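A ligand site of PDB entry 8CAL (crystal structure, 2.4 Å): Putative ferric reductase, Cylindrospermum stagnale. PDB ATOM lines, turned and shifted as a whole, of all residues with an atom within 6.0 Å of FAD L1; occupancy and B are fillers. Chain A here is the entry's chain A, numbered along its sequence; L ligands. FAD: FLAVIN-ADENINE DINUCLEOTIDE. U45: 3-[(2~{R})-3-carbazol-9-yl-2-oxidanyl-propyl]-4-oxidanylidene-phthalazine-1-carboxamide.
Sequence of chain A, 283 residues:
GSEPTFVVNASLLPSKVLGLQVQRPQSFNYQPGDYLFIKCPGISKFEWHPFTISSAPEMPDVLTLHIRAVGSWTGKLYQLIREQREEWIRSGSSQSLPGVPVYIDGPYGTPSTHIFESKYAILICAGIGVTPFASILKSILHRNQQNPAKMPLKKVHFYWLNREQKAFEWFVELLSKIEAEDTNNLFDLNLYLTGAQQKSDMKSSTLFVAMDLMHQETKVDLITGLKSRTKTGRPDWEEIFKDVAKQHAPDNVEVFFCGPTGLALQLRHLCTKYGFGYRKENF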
ATOM      1  N   TYR A  35      -4.532 -18.257  -5.247  1.00  0.00           N
ATOM      2  CA  TYR A  35      -4.834 -16.822  -5.094  1.00  0.00           C
ATOM      3  C   TYR A  35      -4.481 -16.417  -3.658  1.00  0.00           C
ATOM      4  O   TYR A  35      -4.082 -17.276  -2.799  1.00  0.00           O
ATOM      5  CB  TYR A  35      -6.267 -16.552  -5.533  1.00  0.00           C
ATOM      6  CG  TYR A  35      -7.344 -17.179  -4.695  1.00  0.00           C
ATOM      7  CD1 TYR A  35      -7.739 -18.490  -4.877  1.00  0.00           C
ATOM      8  CD2 TYR A  35      -8.017 -16.430  -3.737  1.00  0.00           C
ATOM      9  CE1 TYR A  35      -8.743 -19.050  -4.095  1.00  0.00           C
ATOM     10  CE2 TYR A  35      -9.038 -16.969  -2.972  1.00  0.00           C
ATOM     11  CZ  TYR A  35      -9.403 -18.280  -3.158  1.00  0.00           C
ATOM     12  OH  TYR A  35     -10.417 -18.798  -2.427  1.00  0.00           O
ATOM     13  N   GLU A  47     -10.945  -3.534   3.942  1.00  0.00           N
ATOM     14  CA  GLU A  47     -11.403  -4.383   2.812  1.00  0.00           C
ATOM     15  C   GLU A  47     -10.254  -5.290   2.355  1.00  0.00           C
ATOM     16  O   GLU A  47      -9.150  -4.808   2.269  1.00  0.00           O
ATOM     17  CB  GLU A  47     -11.839  -3.567   1.610  1.00  0.00           C
ATOM     18  CG  GLU A  47     -13.248  -3.075   1.680  1.00  0.00           C
ATOM     19  CD  GLU A  47     -13.866  -2.646   0.369  1.00  0.00           C
ATOM     20  OE1 GLU A  47     -13.118  -2.431  -0.638  1.00  0.00           O
ATOM     21  OE2 GLU A  47     -15.096  -2.468   0.341  1.00  0.00           O
ATOM     22  N   HIS A  49      -9.467  -7.997  -0.842  1.00  0.00           N
ATOM     23  CA  HIS A  49      -9.868  -8.448  -2.180  1.00  0.00           C
ATOM     24  C   HIS A  49      -8.947  -9.575  -2.643  1.00  0.00           C
ATOM     25  O   HIS A  49      -7.768  -9.619  -2.325  1.00  0.00           O
ATOM     26  CB  HIS A  49      -9.922  -7.317  -3.176  1.00  0.00           C
ATOM     27  CG  HIS A  49     -10.997  -6.327  -2.950  1.00  0.00           C
ATOM     28  ND1 HIS A  49     -12.101  -6.263  -3.773  1.00  0.00           N
ATOM     29  CD2 HIS A  49     -11.086  -5.302  -2.065  1.00  0.00           C
ATOM     30  CE1 HIS A  49     -12.842  -5.232  -3.395  1.00  0.00           C
ATOM     31  NE2 HIS A  49     -12.238  -4.624  -2.344  1.00  0.00           N
ATOM     32  N   PRO A  50      -9.539 -10.600  -3.276  1.00  0.00           N
ATOM     33  CA  PRO A  50      -8.772 -11.743  -3.760  1.00  0.00           C
ATOM     34  C   PRO A  50      -8.196 -11.512  -5.171  1.00  0.00           C
ATOM     35  O   PRO A  50      -8.866 -10.986  -6.075  1.00  0.00           O
ATOM     36  CB  PRO A  50      -9.836 -12.828  -3.771  1.00  0.00           C
ATOM     37  CG  PRO A  50     -11.108 -12.088  -4.180  1.00  0.00           C
ATOM     38  CD  PRO A  50     -11.000 -10.734  -3.495  1.00  0.00           C
ATOM     39  N   PHE A  51      -6.949 -11.900  -5.347  1.00  0.00           N
ATOM     40  CA  PHE A  51      -6.306 -11.853  -6.678  1.00  0.00           C
ATOM     41  C   PHE A  51      -5.478 -13.124  -6.830  1.00  0.00           C
ATOM     42  O   PHE A  51      -4.841 -13.591  -5.839  1.00  0.00           O
ATOM     43  CB  PHE A  51      -5.502 -10.564  -6.860  1.00  0.00           C
ATOM     44  CG  PHE A  51      -6.329  -9.312  -6.792  1.00  0.00           C
ATOM     45  CD1 PHE A  51      -7.130  -8.921  -7.843  1.00  0.00           C
ATOM     46  CD2 PHE A  51      -6.355  -8.535  -5.646  1.00  0.00           C
ATOM     47  CE1 PHE A  51      -7.940  -7.792  -7.746  1.00  0.00           C
ATOM     48  CE2 PHE A  51      -7.173  -7.420  -5.530  1.00  0.00           C
ATOM     49  CZ  PHE A  51      -7.975  -7.053  -6.580  1.00  0.00           C
ATOM     50  N   THR A  52      -5.549 -13.696  -8.029  1.00  0.00           N
ATOM     51  CA  THR A  52      -4.686 -14.814  -8.454  1.00  0.00           C
ATOM     52  C   THR A  52      -3.245 -14.326  -8.402  1.00  0.00           C
ATOM     53  O   THR A  52      -2.969 -13.181  -8.860  1.00  0.00           O
ATOM     54  CB  THR A  52      -5.006 -15.235  -9.894  1.00  0.00           C
ATOM     55  OG1 THR A  52      -6.387 -15.586 -10.022  1.00  0.00           O
ATOM     56  CG2 THR A  52      -4.104 -16.368 -10.311  1.00  0.00           C
ATOM     57  N   ILE A  53      -2.363 -15.166  -7.922  1.00  0.00           N
ATOM     58  CA  ILE A  53      -0.907 -14.970  -8.123  1.00  0.00           C
ATOM     59  C   ILE A  53      -0.510 -15.355  -9.566  1.00  0.00           C
ATOM     60  O   ILE A  53      -0.352 -16.549  -9.854  1.00  0.00           O
ATOM     61  CB  ILE A  53      -0.151 -15.820  -7.111  1.00  0.00           C
ATOM     62  CG1 ILE A  53      -0.672 -15.576  -5.703  1.00  0.00           C
ATOM     63  CG2 ILE A  53       1.342 -15.572  -7.237  1.00  0.00           C
ATOM     64  CD1 ILE A  53      -0.013 -16.461  -4.673  1.00  0.00           C
ATOM     65  N   HIS A  66      -1.896  -9.344 -11.397  1.00  0.00           N
ATOM     66  CA  HIS A  66      -2.407  -8.521 -12.493  1.00  0.00           C
ATOM     67  C   HIS A  66      -3.830  -8.171 -12.152  1.00  0.00           C
ATOM     68  O   HIS A  66      -4.681  -9.028 -12.275  1.00  0.00           O
ATOM     69  CB  HIS A  66      -2.315  -9.237 -13.836  1.00  0.00           C
ATOM     70  CG  HIS A  66      -0.926  -9.326 -14.341  1.00  0.00           C
ATOM     71  ND1 HIS A  66      -0.009 -10.187 -13.767  1.00  0.00           N
ATOM     72  CD2 HIS A  66      -0.293  -8.669 -15.343  1.00  0.00           C
ATOM     73  CE1 HIS A  66       1.135 -10.076 -14.411  1.00  0.00           C
ATOM     74  NE2 HIS A  66       0.994  -9.110 -15.357  1.00  0.00           N
ATOM     75  N   ILE A  67      -4.044  -6.907 -11.836  1.00  0.00           N
ATOM     76  CA  ILE A  67      -5.312  -6.370 -11.300  1.00  0.00           C
ATOM     77  C   ILE A  67      -5.874  -5.387 -12.290  1.00  0.00           C
ATOM     78  O   ILE A  67      -5.193  -4.417 -12.591  1.00  0.00           O
ATOM     79  CB  ILE A  67      -5.007  -5.692  -9.956  1.00  0.00           C
ATOM     80  CG1 ILE A  67      -4.347  -6.669  -8.990  1.00  0.00           C
ATOM     81  CG2 ILE A  67      -6.292  -5.076  -9.423  1.00  0.00           C
ATOM     82  CD1 ILE A  67      -4.157  -6.108  -7.633  1.00  0.00           C
ATOM     83  N   ARG A  68      -7.071  -5.654 -12.763  1.00  0.00           N
ATOM     84  CA  ARG A  68      -7.830  -4.740 -13.647  1.00  0.00           C
ATOM     85  C   ARG A  68      -8.745  -3.816 -12.812  1.00  0.00           C
ATOM     86  O   ARG A  68      -9.521  -4.284 -11.973  1.00  0.00           O
ATOM     87  CB  ARG A  68      -8.582  -5.593 -14.665  1.00  0.00           C
ATOM     88  CG  ARG A  68      -9.286  -4.776 -15.728  1.00  0.00           C
ATOM     89  CD  ARG A  68      -9.544  -5.609 -16.955  1.00  0.00           C
ATOM     90  NE  ARG A  68     -10.032  -4.708 -17.971  1.00  0.00           N
ATOM     91  CZ  ARG A  68     -11.286  -4.563 -18.286  1.00  0.00           C
ATOM     92  NH1 ARG A  68     -12.211  -5.284 -17.697  1.00  0.00           N
ATOM     93  NH2 ARG A  68     -11.620  -3.690 -19.219  1.00  0.00           N
ATOM     94  N   ALA A  69      -8.682  -2.516 -13.098  1.00  0.00           N
ATOM     95  CA  ALA A  69      -9.536  -1.443 -12.561  1.00  0.00           C
ATOM     96  C   ALA A  69     -10.940  -1.630 -13.091  1.00  0.00           C
ATOM     97  O   ALA A  69     -11.145  -1.210 -14.210  1.00  0.00           O
ATOM     98  CB  ALA A  69      -9.015  -0.089 -12.967  1.00  0.00           C
ATOM     99  N   VAL A  70     -11.851  -2.163 -12.287  1.00  0.00           N
ATOM    100  CA  VAL A  70     -13.269  -2.445 -12.670  1.00  0.00           C
ATOM    101  C   VAL A  70     -14.258  -1.745 -11.735  1.00  0.00           C
ATOM    102  O   VAL A  70     -15.427  -1.801 -12.014  1.00  0.00           O
ATOM    103  CB  VAL A  70     -13.545  -3.965 -12.647  1.00  0.00           C
ATOM    104  CG1 VAL A  70     -12.703  -4.664 -13.684  1.00  0.00           C
ATOM    105  CG2 VAL A  70     -13.292  -4.548 -11.251  1.00  0.00           C
ATOM    106  N   GLY A  71     -13.836  -1.280 -10.566  1.00  0.00           N
ATOM    107  CA  GLY A  71     -14.731  -0.495  -9.702  1.00  0.00           C
ATOM    108  C   GLY A  71     -14.002   0.192  -8.568  1.00  0.00           C
ATOM    109  O   GLY A  71     -12.839   0.578  -8.713  1.00  0.00           O
ATOM    110  N   SER A  72     -14.673   0.297  -7.431  1.00  0.00           N
ATOM    111  CA  SER A  72     -14.269   1.177  -6.334  1.00  0.00           C
ATOM    112  C   SER A  72     -12.811   0.881  -5.981  1.00  0.00           C
ATOM    113  O   SER A  72     -11.970   1.749  -6.213  1.00  0.00           O
ATOM    114  CB  SER A  72     -15.226   1.041  -5.169  1.00  0.00           C
ATOM    115  OG  SER A  72     -14.690   1.700  -4.024  1.00  0.00           O
ATOM    116  N   TRP A  73     -12.504  -0.271  -5.392  1.00  0.00           N
ATOM    117  CA  TRP A  73     -11.196  -0.539  -4.750  1.00  0.00           C
ATOM    118  C   TRP A  73     -10.066  -0.667  -5.782  1.00  0.00           C
ATOM    119  O   TRP A  73      -9.000  -0.092  -5.552  1.00  0.00           O
ATOM    120  CB  TRP A  73     -11.305  -1.796  -3.904  1.00  0.00           C
ATOM    121  CG  TRP A  73     -10.133  -2.097  -3.030  1.00  0.00           C
ATOM    122  CD1 TRP A  73     -10.051  -1.885  -1.698  1.00  0.00           C
ATOM    123  CD2 TRP A  73      -8.947  -2.810  -3.389  1.00  0.00           C
ATOM    124  NE1 TRP A  73      -8.874  -2.355  -1.200  1.00  0.00           N
ATOM    125  CE2 TRP A  73      -8.174  -2.922  -2.223  1.00  0.00           C
ATOM    126  CE3 TRP A  73      -8.451  -3.332  -4.591  1.00  0.00           C
ATOM    127  CZ2 TRP A  73      -6.911  -3.524  -2.221  1.00  0.00           C
ATOM    128  CZ3 TRP A  73      -7.201  -3.937  -4.590  1.00  0.00           C
ATOM    129  CH2 TRP A  73      -6.443  -4.023  -3.420  1.00  0.00           C
ATOM    130  N   THR A  74     -10.267  -1.424  -6.860  1.00  0.00           N
ATOM    131  CA  THR A  74      -9.263  -1.571  -7.963  1.00  0.00           C
ATOM    132  C   THR A  74      -9.037  -0.196  -8.632  1.00  0.00           C
ATOM    133  O   THR A  74      -7.877   0.148  -8.896  1.00  0.00           O
ATOM    134  CB  THR A  74      -9.652  -2.672  -8.973  1.00  0.00           C
ATOM    135  OG1 THR A  74     -10.966  -2.469  -9.518  1.00  0.00           O
ATOM    136  CG2 THR A  74      -9.610  -4.037  -8.344  1.00  0.00           C
ATOM    137  N   GLY A  75     -10.107   0.566  -8.903  1.00  0.00           N
ATOM    138  CA  GLY A  75      -9.980   1.946  -9.410  1.00  0.00           C
ATOM    139  C   GLY A  75      -9.067   2.790  -8.533  1.00  0.00           C
ATOM    140  O   GLY A  75      -8.156   3.450  -9.029  1.00  0.00           O
ATOM    141  N   THR A 110      -7.081 -23.673  -5.794  1.00  0.00           N
ATOM    142  CA  THR A 110      -8.145 -23.792  -6.808  1.00  0.00           C
ATOM    143  C   THR A 110      -7.932 -25.152  -7.425  1.00  0.00           C
ATOM    144  O   THR A 110      -6.807 -25.671  -7.355  1.00  0.00           O
ATOM    145  CB  THR A 110      -8.131 -22.688  -7.877  1.00  0.00           C
ATOM    146  OG1 THR A 110      -6.971 -22.790  -8.701  1.00  0.00           O
ATOM    147  CG2 THR A 110      -8.180 -21.301  -7.266  1.00  0.00           C
ATOM    148  N   ILE A 128      -9.082 -10.992 -17.868  1.00  0.00           N
ATOM    149  CA  ILE A 128      -8.045 -11.085 -16.795  1.00  0.00           C
ATOM    150  C   ILE A 128      -8.116 -12.483 -16.142  1.00  0.00           C
ATOM    151  O   ILE A 128      -7.181 -12.862 -15.382  1.00  0.00           O
ATOM    152  CB  ILE A 128      -8.219  -9.919 -15.789  1.00  0.00           C
ATOM    153  CG1 ILE A 128      -6.959  -9.698 -14.973  1.00  0.00           C
ATOM    154  CG2 ILE A 128      -9.425 -10.140 -14.894  1.00  0.00           C
ATOM    155  CD1 ILE A 128      -5.836  -9.162 -15.779  1.00  0.00           C
ATOM    156  N   THR A 131      -5.128 -15.106 -15.646  1.00  0.00           N
ATOM    157  CA  THR A 131      -4.013 -14.992 -14.675  1.00  0.00           C
ATOM    158  C   THR A 131      -3.651 -16.340 -14.062  1.00  0.00           C
ATOM    159  O   THR A 131      -2.471 -16.610 -13.849  1.00  0.00           O
ATOM    160  CB  THR A 131      -4.317 -13.905 -13.658  1.00  0.00           C
ATOM    161  OG1 THR A 131      -5.605 -14.140 -13.088  1.00  0.00           O
ATOM    162  CG2 THR A 131      -4.335 -12.550 -14.335  1.00  0.00           C
ATOM    163  N   PRO A 132      -4.582 -17.214 -13.647  1.00  0.00           N
ATOM    164  CA  PRO A 132      -4.143 -18.456 -13.016  1.00  0.00           C
ATOM    165  C   PRO A 132      -3.438 -19.311 -14.083  1.00  0.00           C
ATOM    166  O   PRO A 132      -2.497 -20.009 -13.778  1.00  0.00           O
ATOM    167  CB  PRO A 132      -5.436 -19.032 -12.437  1.00  0.00           C
ATOM    168  CG  PRO A 132      -6.538 -18.443 -13.283  1.00  0.00           C
ATOM    169  CD  PRO A 132      -6.035 -17.083 -13.675  1.00  0.00           C
HETATM  170  PA  FAD L   1     -16.588  -3.271  -7.450  1.00  0.00           P
HETATM  171  O1A FAD L   1     -16.964  -4.386  -6.548  1.00  0.00           O
HETATM  172  O2A FAD L   1     -16.826  -1.822  -7.156  1.00  0.00           O
HETATM  173  O5B FAD L   1     -17.278  -3.596  -8.859  1.00  0.00           O
HETATM  174  C5B FAD L   1     -17.193  -4.923  -9.448  1.00  0.00           C
HETATM  175  C4B FAD L   1     -18.140  -5.006 -10.618  1.00  0.00           C
HETATM  176  O4B FAD L   1     -19.517  -5.055 -10.135  1.00  0.00           O
HETATM  177  C3B FAD L   1     -18.114  -3.822 -11.588  1.00  0.00           C
HETATM  178  O3B FAD L   1     -18.408  -4.272 -12.908  1.00  0.00           O
HETATM  179  C2B FAD L   1     -19.197  -2.906 -10.997  1.00  0.00           C
HETATM  180  O2B FAD L   1     -19.804  -2.032 -11.911  1.00  0.00           O
HETATM  181  C1B FAD L   1     -20.224  -3.922 -10.561  1.00  0.00           C
HETATM  182  N9A FAD L   1     -21.065  -3.438  -9.492  1.00  0.00           N
HETATM  183  C8A FAD L   1     -20.683  -2.786  -8.338  1.00  0.00           C
HETATM  184  N7A FAD L   1     -21.715  -2.454  -7.591  1.00  0.00           N
HETATM  185  C5A FAD L   1     -22.813  -2.904  -8.310  1.00  0.00           C
HETATM  186  C6A FAD L   1     -24.200  -2.855  -8.056  1.00  0.00           C
HETATM  187  N6A FAD L   1     -24.710  -2.288  -6.980  1.00  0.00           N
HETATM  188  N1A FAD L   1     -25.032  -3.410  -8.985  1.00  0.00           N
HETATM  189  C2A FAD L   1     -24.497  -3.976 -10.079  1.00  0.00           C
HETATM  190  N3A FAD L   1     -23.212  -4.068 -10.420  1.00  0.00           N
HETATM  191  C4A FAD L   1     -22.424  -3.518  -9.488  1.00  0.00           C
HETATM  192  N1  FAD L   1      -9.342  -9.644 -10.612  1.00  0.00           N
HETATM  193  C2  FAD L   1      -8.250  -9.299 -11.313  1.00  0.00           C
HETATM  194  O2  FAD L   1      -8.226  -8.221 -11.850  1.00  0.00           O
HETATM  195  N3  FAD L   1      -7.149 -10.110 -11.435  1.00  0.00           N
HETATM  196  C4  FAD L   1      -7.104 -11.352 -10.866  1.00  0.00           C
HETATM  197  O4  FAD L   1      -6.119 -12.053 -11.014  1.00  0.00           O
HETATM  198  C4X FAD L   1      -8.216 -11.730 -10.079  1.00  0.00           C
HETATM  199  N5  FAD L   1      -8.175 -12.889  -9.512  1.00  0.00           N
HETATM  200  C5X FAD L   1      -9.263 -13.218  -8.759  1.00  0.00           C
HETATM  201  C6  FAD L   1      -9.209 -14.463  -8.102  1.00  0.00           C
HETATM  202  C7  FAD L   1     -10.222 -14.918  -7.313  1.00  0.00           C
HETATM  203  C7M FAD L   1     -10.092 -16.276  -6.652  1.00  0.00           C
HETATM  204  C8  FAD L   1     -11.352 -14.117  -7.134  1.00  0.00           C
HETATM  205  C8M FAD L   1     -12.493 -14.623  -6.291  1.00  0.00           C
HETATM  206  C9  FAD L   1     -11.447 -12.881  -7.797  1.00  0.00           C
HETATM  207  C9A FAD L   1     -10.408 -12.389  -8.612  1.00  0.00           C
HETATM  208  N10 FAD L   1     -10.424 -11.130  -9.255  1.00  0.00           N
HETATM  209  C10 FAD L   1      -9.327 -10.789  -9.989  1.00  0.00           C
HETATM  210  C1' FAD L   1     -11.514 -10.089  -9.064  1.00  0.00           C
HETATM  211  C2' FAD L   1     -11.249  -9.162  -7.783  1.00  0.00           C
HETATM  212  O2' FAD L   1     -11.056 -10.053  -6.663  1.00  0.00           O
HETATM  213  C3' FAD L   1     -11.977  -7.895  -7.205  1.00  0.00           C
HETATM  214  O3' FAD L   1     -12.880  -7.734  -6.022  1.00  0.00           O
HETATM  215  C4' FAD L   1     -12.916  -7.269  -8.172  1.00  0.00           C
HETATM  216  O4' FAD L   1     -12.374  -7.846  -9.353  1.00  0.00           O
HETATM  217  C5' FAD L   1     -12.876  -5.768  -7.963  1.00  0.00           C
HETATM  218  O5' FAD L   1     -13.418  -5.157  -6.730  1.00  0.00           O
HETATM  219  P   FAD L   1     -13.748  -3.534  -6.780  1.00  0.00           P
HETATM  220  O1P FAD L   1     -14.107  -2.967  -5.483  1.00  0.00           O
HETATM  221  O2P FAD L   1     -12.650  -2.835  -7.522  1.00  0.00           O
HETATM  222  O3P FAD L   1     -15.019  -3.431  -7.720  1.00  0.00           O
HETATM  223  CAM U45 L   2     -13.385 -12.088 -11.542  1.00  0.00           C
HETATM  224  CAL U45 L   2     -14.704 -11.904 -11.062  1.00  0.00           C
HETATM  225  CAT U45 L   2     -15.266 -12.954 -10.285  1.00  0.00           C
HETATM  226  CAJ U45 L   2     -14.509 -14.135  -9.984  1.00  0.00           C
HETATM  227  CAS U45 L   2     -13.239 -14.236 -10.456  1.00  0.00           C
HETATM  228  CAN U45 L   2     -12.703 -13.239 -11.220  1.00  0.00           C
HETATM  229  CAO U45 L   2     -11.450 -13.619 -11.543  1.00  0.00           C
HETATM  230  CAP U45 L   2     -10.517 -12.971 -12.277  1.00  0.00           C
HETATM  231  CAQ U45 L   2      -9.263 -13.575 -12.516  1.00  0.00           C
HETATM  232  CAU U45 L   2      -9.027 -14.832 -11.932  1.00  0.00           C
HETATM  233  CAV U45 L   2     -10.048 -15.466 -11.171  1.00  0.00           C
HETATM  234  CBC U45 L   2     -11.228 -14.854 -11.001  1.00  0.00           C
HETATM  235  NAR U45 L   2     -12.319 -15.221 -10.322  1.00  0.00           N
HETATM  236  CAK U45 L   2     -12.617 -16.474  -9.590  1.00  0.00           C
HETATM  237  CAH U45 L   2     -13.753 -17.234 -10.472  1.00  0.00           C
HETATM  238  OAI U45 L   2     -12.896 -18.016 -11.336  1.00  0.00           O
HETATM  239  CAD U45 L   2     -14.906 -18.164  -9.859  1.00  0.00           C
HETATM  240  NAG U45 L   2     -14.497 -18.242  -8.456  1.00  0.00           N
HETATM  241  NAF U45 L   2     -13.516 -18.956  -8.250  1.00  0.00           N
HETATM  242  CBD U45 L   2     -15.143 -17.462  -7.532  1.00  0.00           C
HETATM  243  OBE U45 L   2     -16.148 -16.745  -7.782  1.00  0.00           O
HETATM  244  CAW U45 L   2     -14.641 -17.459  -6.247  1.00  0.00           C
HETATM  245  CAX U45 L   2     -15.281 -16.631  -5.290  1.00  0.00           C
HETATM  246  CAY U45 L   2     -14.808 -16.600  -3.994  1.00  0.00           C
HETATM  247  CAZ U45 L   2     -13.690 -17.393  -3.703  1.00  0.00           C
HETATM  248  CBA U45 L   2     -13.092 -18.231  -4.666  1.00  0.00           C
HETATM  249  CBB U45 L   2     -13.556 -18.259  -5.973  1.00  0.00           C
HETATM  250  CAE U45 L   2     -12.987 -19.016  -7.004  1.00  0.00           C
HETATM  251  CAB U45 L   2     -11.961 -19.935  -6.892  1.00  0.00           C
HETATM  252  OAC U45 L   2     -11.152 -19.852  -5.986  1.00  0.00           O
HETATM  253  NAA U45 L   2     -12.071 -21.076  -7.692  1.00  0.00           N
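The backbone NH (N) of Arg 68 sits at hydrogen-bond distance from an oxygen (O2) of FAD L1 (3.0 Å).
N of Thr 74 sits at hydrogen-bond distance from O2P of FAD L1, at 2.8 Å.
A nitrogen (N5) of FAD L1 sits at hydrogen-bond distance from the side-chain hydroxyl (OG1) of Thr 52 (3.3 Å).
O of His 66 sits at hydrogen-bond distance from N3 of FAD L1.
A nitrogen (N5) of FAD L1 is in hydrogen-bond range of the backbone NH of Thr 52 (3.1 Å).
An oxygen (O1P) of FAD L1 is in hydrogen-bond range of the backbone NH (N) of Trp 73, at 3.1 Å.
O of Pro 50 is in hydrogen-bond range of O2' of FAD L1, at 2.5 Å.
An oxygen (O3') of FAD L1 sits at hydrogen-bond distance from a ring nitrogen (ND1) of His 49 (2.8 Å).
OG1 of Thr 74 lies within hydrogen-bond range of O2P of FAD L1.
An oxygen (O2A) of FAD L1 sits at hydrogen-bond distance from the backbone NH (N) of Ser 72 (3.0 Å).
An oxygen (O4) of FAD L1 is in hydrogen-bond range of the side-chain hydroxyl of Thr 131 (3.0 Å).
OG1 of Thr 74 lies within hydrogen-bond range of N of Gly 71 (3.3 Å).
A ring nitrogen (NE2) of His 49 sits at hydrogen-bond distance from the side-chain carboxylate (OE1) of Glu 47.
OG1 of Thr 74 is in hydrogen-bond range of O of Arg 68, 3.4 Å away.
OG1 of Thr 74 lies within hydrogen-bond range of N of Val 70 (2.9 Å).
OG1 of Thr 52 lies close to OG1 of Thr 131, at 3.5 Å.
The backbone carbonyl oxygen (O) of Ile 128 lies close to the side-chain hydroxyl (OG1) of Thr 131 (3.1 Å).
Merely in contact with FAD L1: Val 70 (3.4 Å), Gly 71 (3.5 Å), Tyr 35 (3.5 Å), Ile 67 (3.5 Å), Phe 51 (3.5 Å) and Ile 128 (3.6 Å).
Of the 21 residues printed, 15 come within 4 Å of FAD L1.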
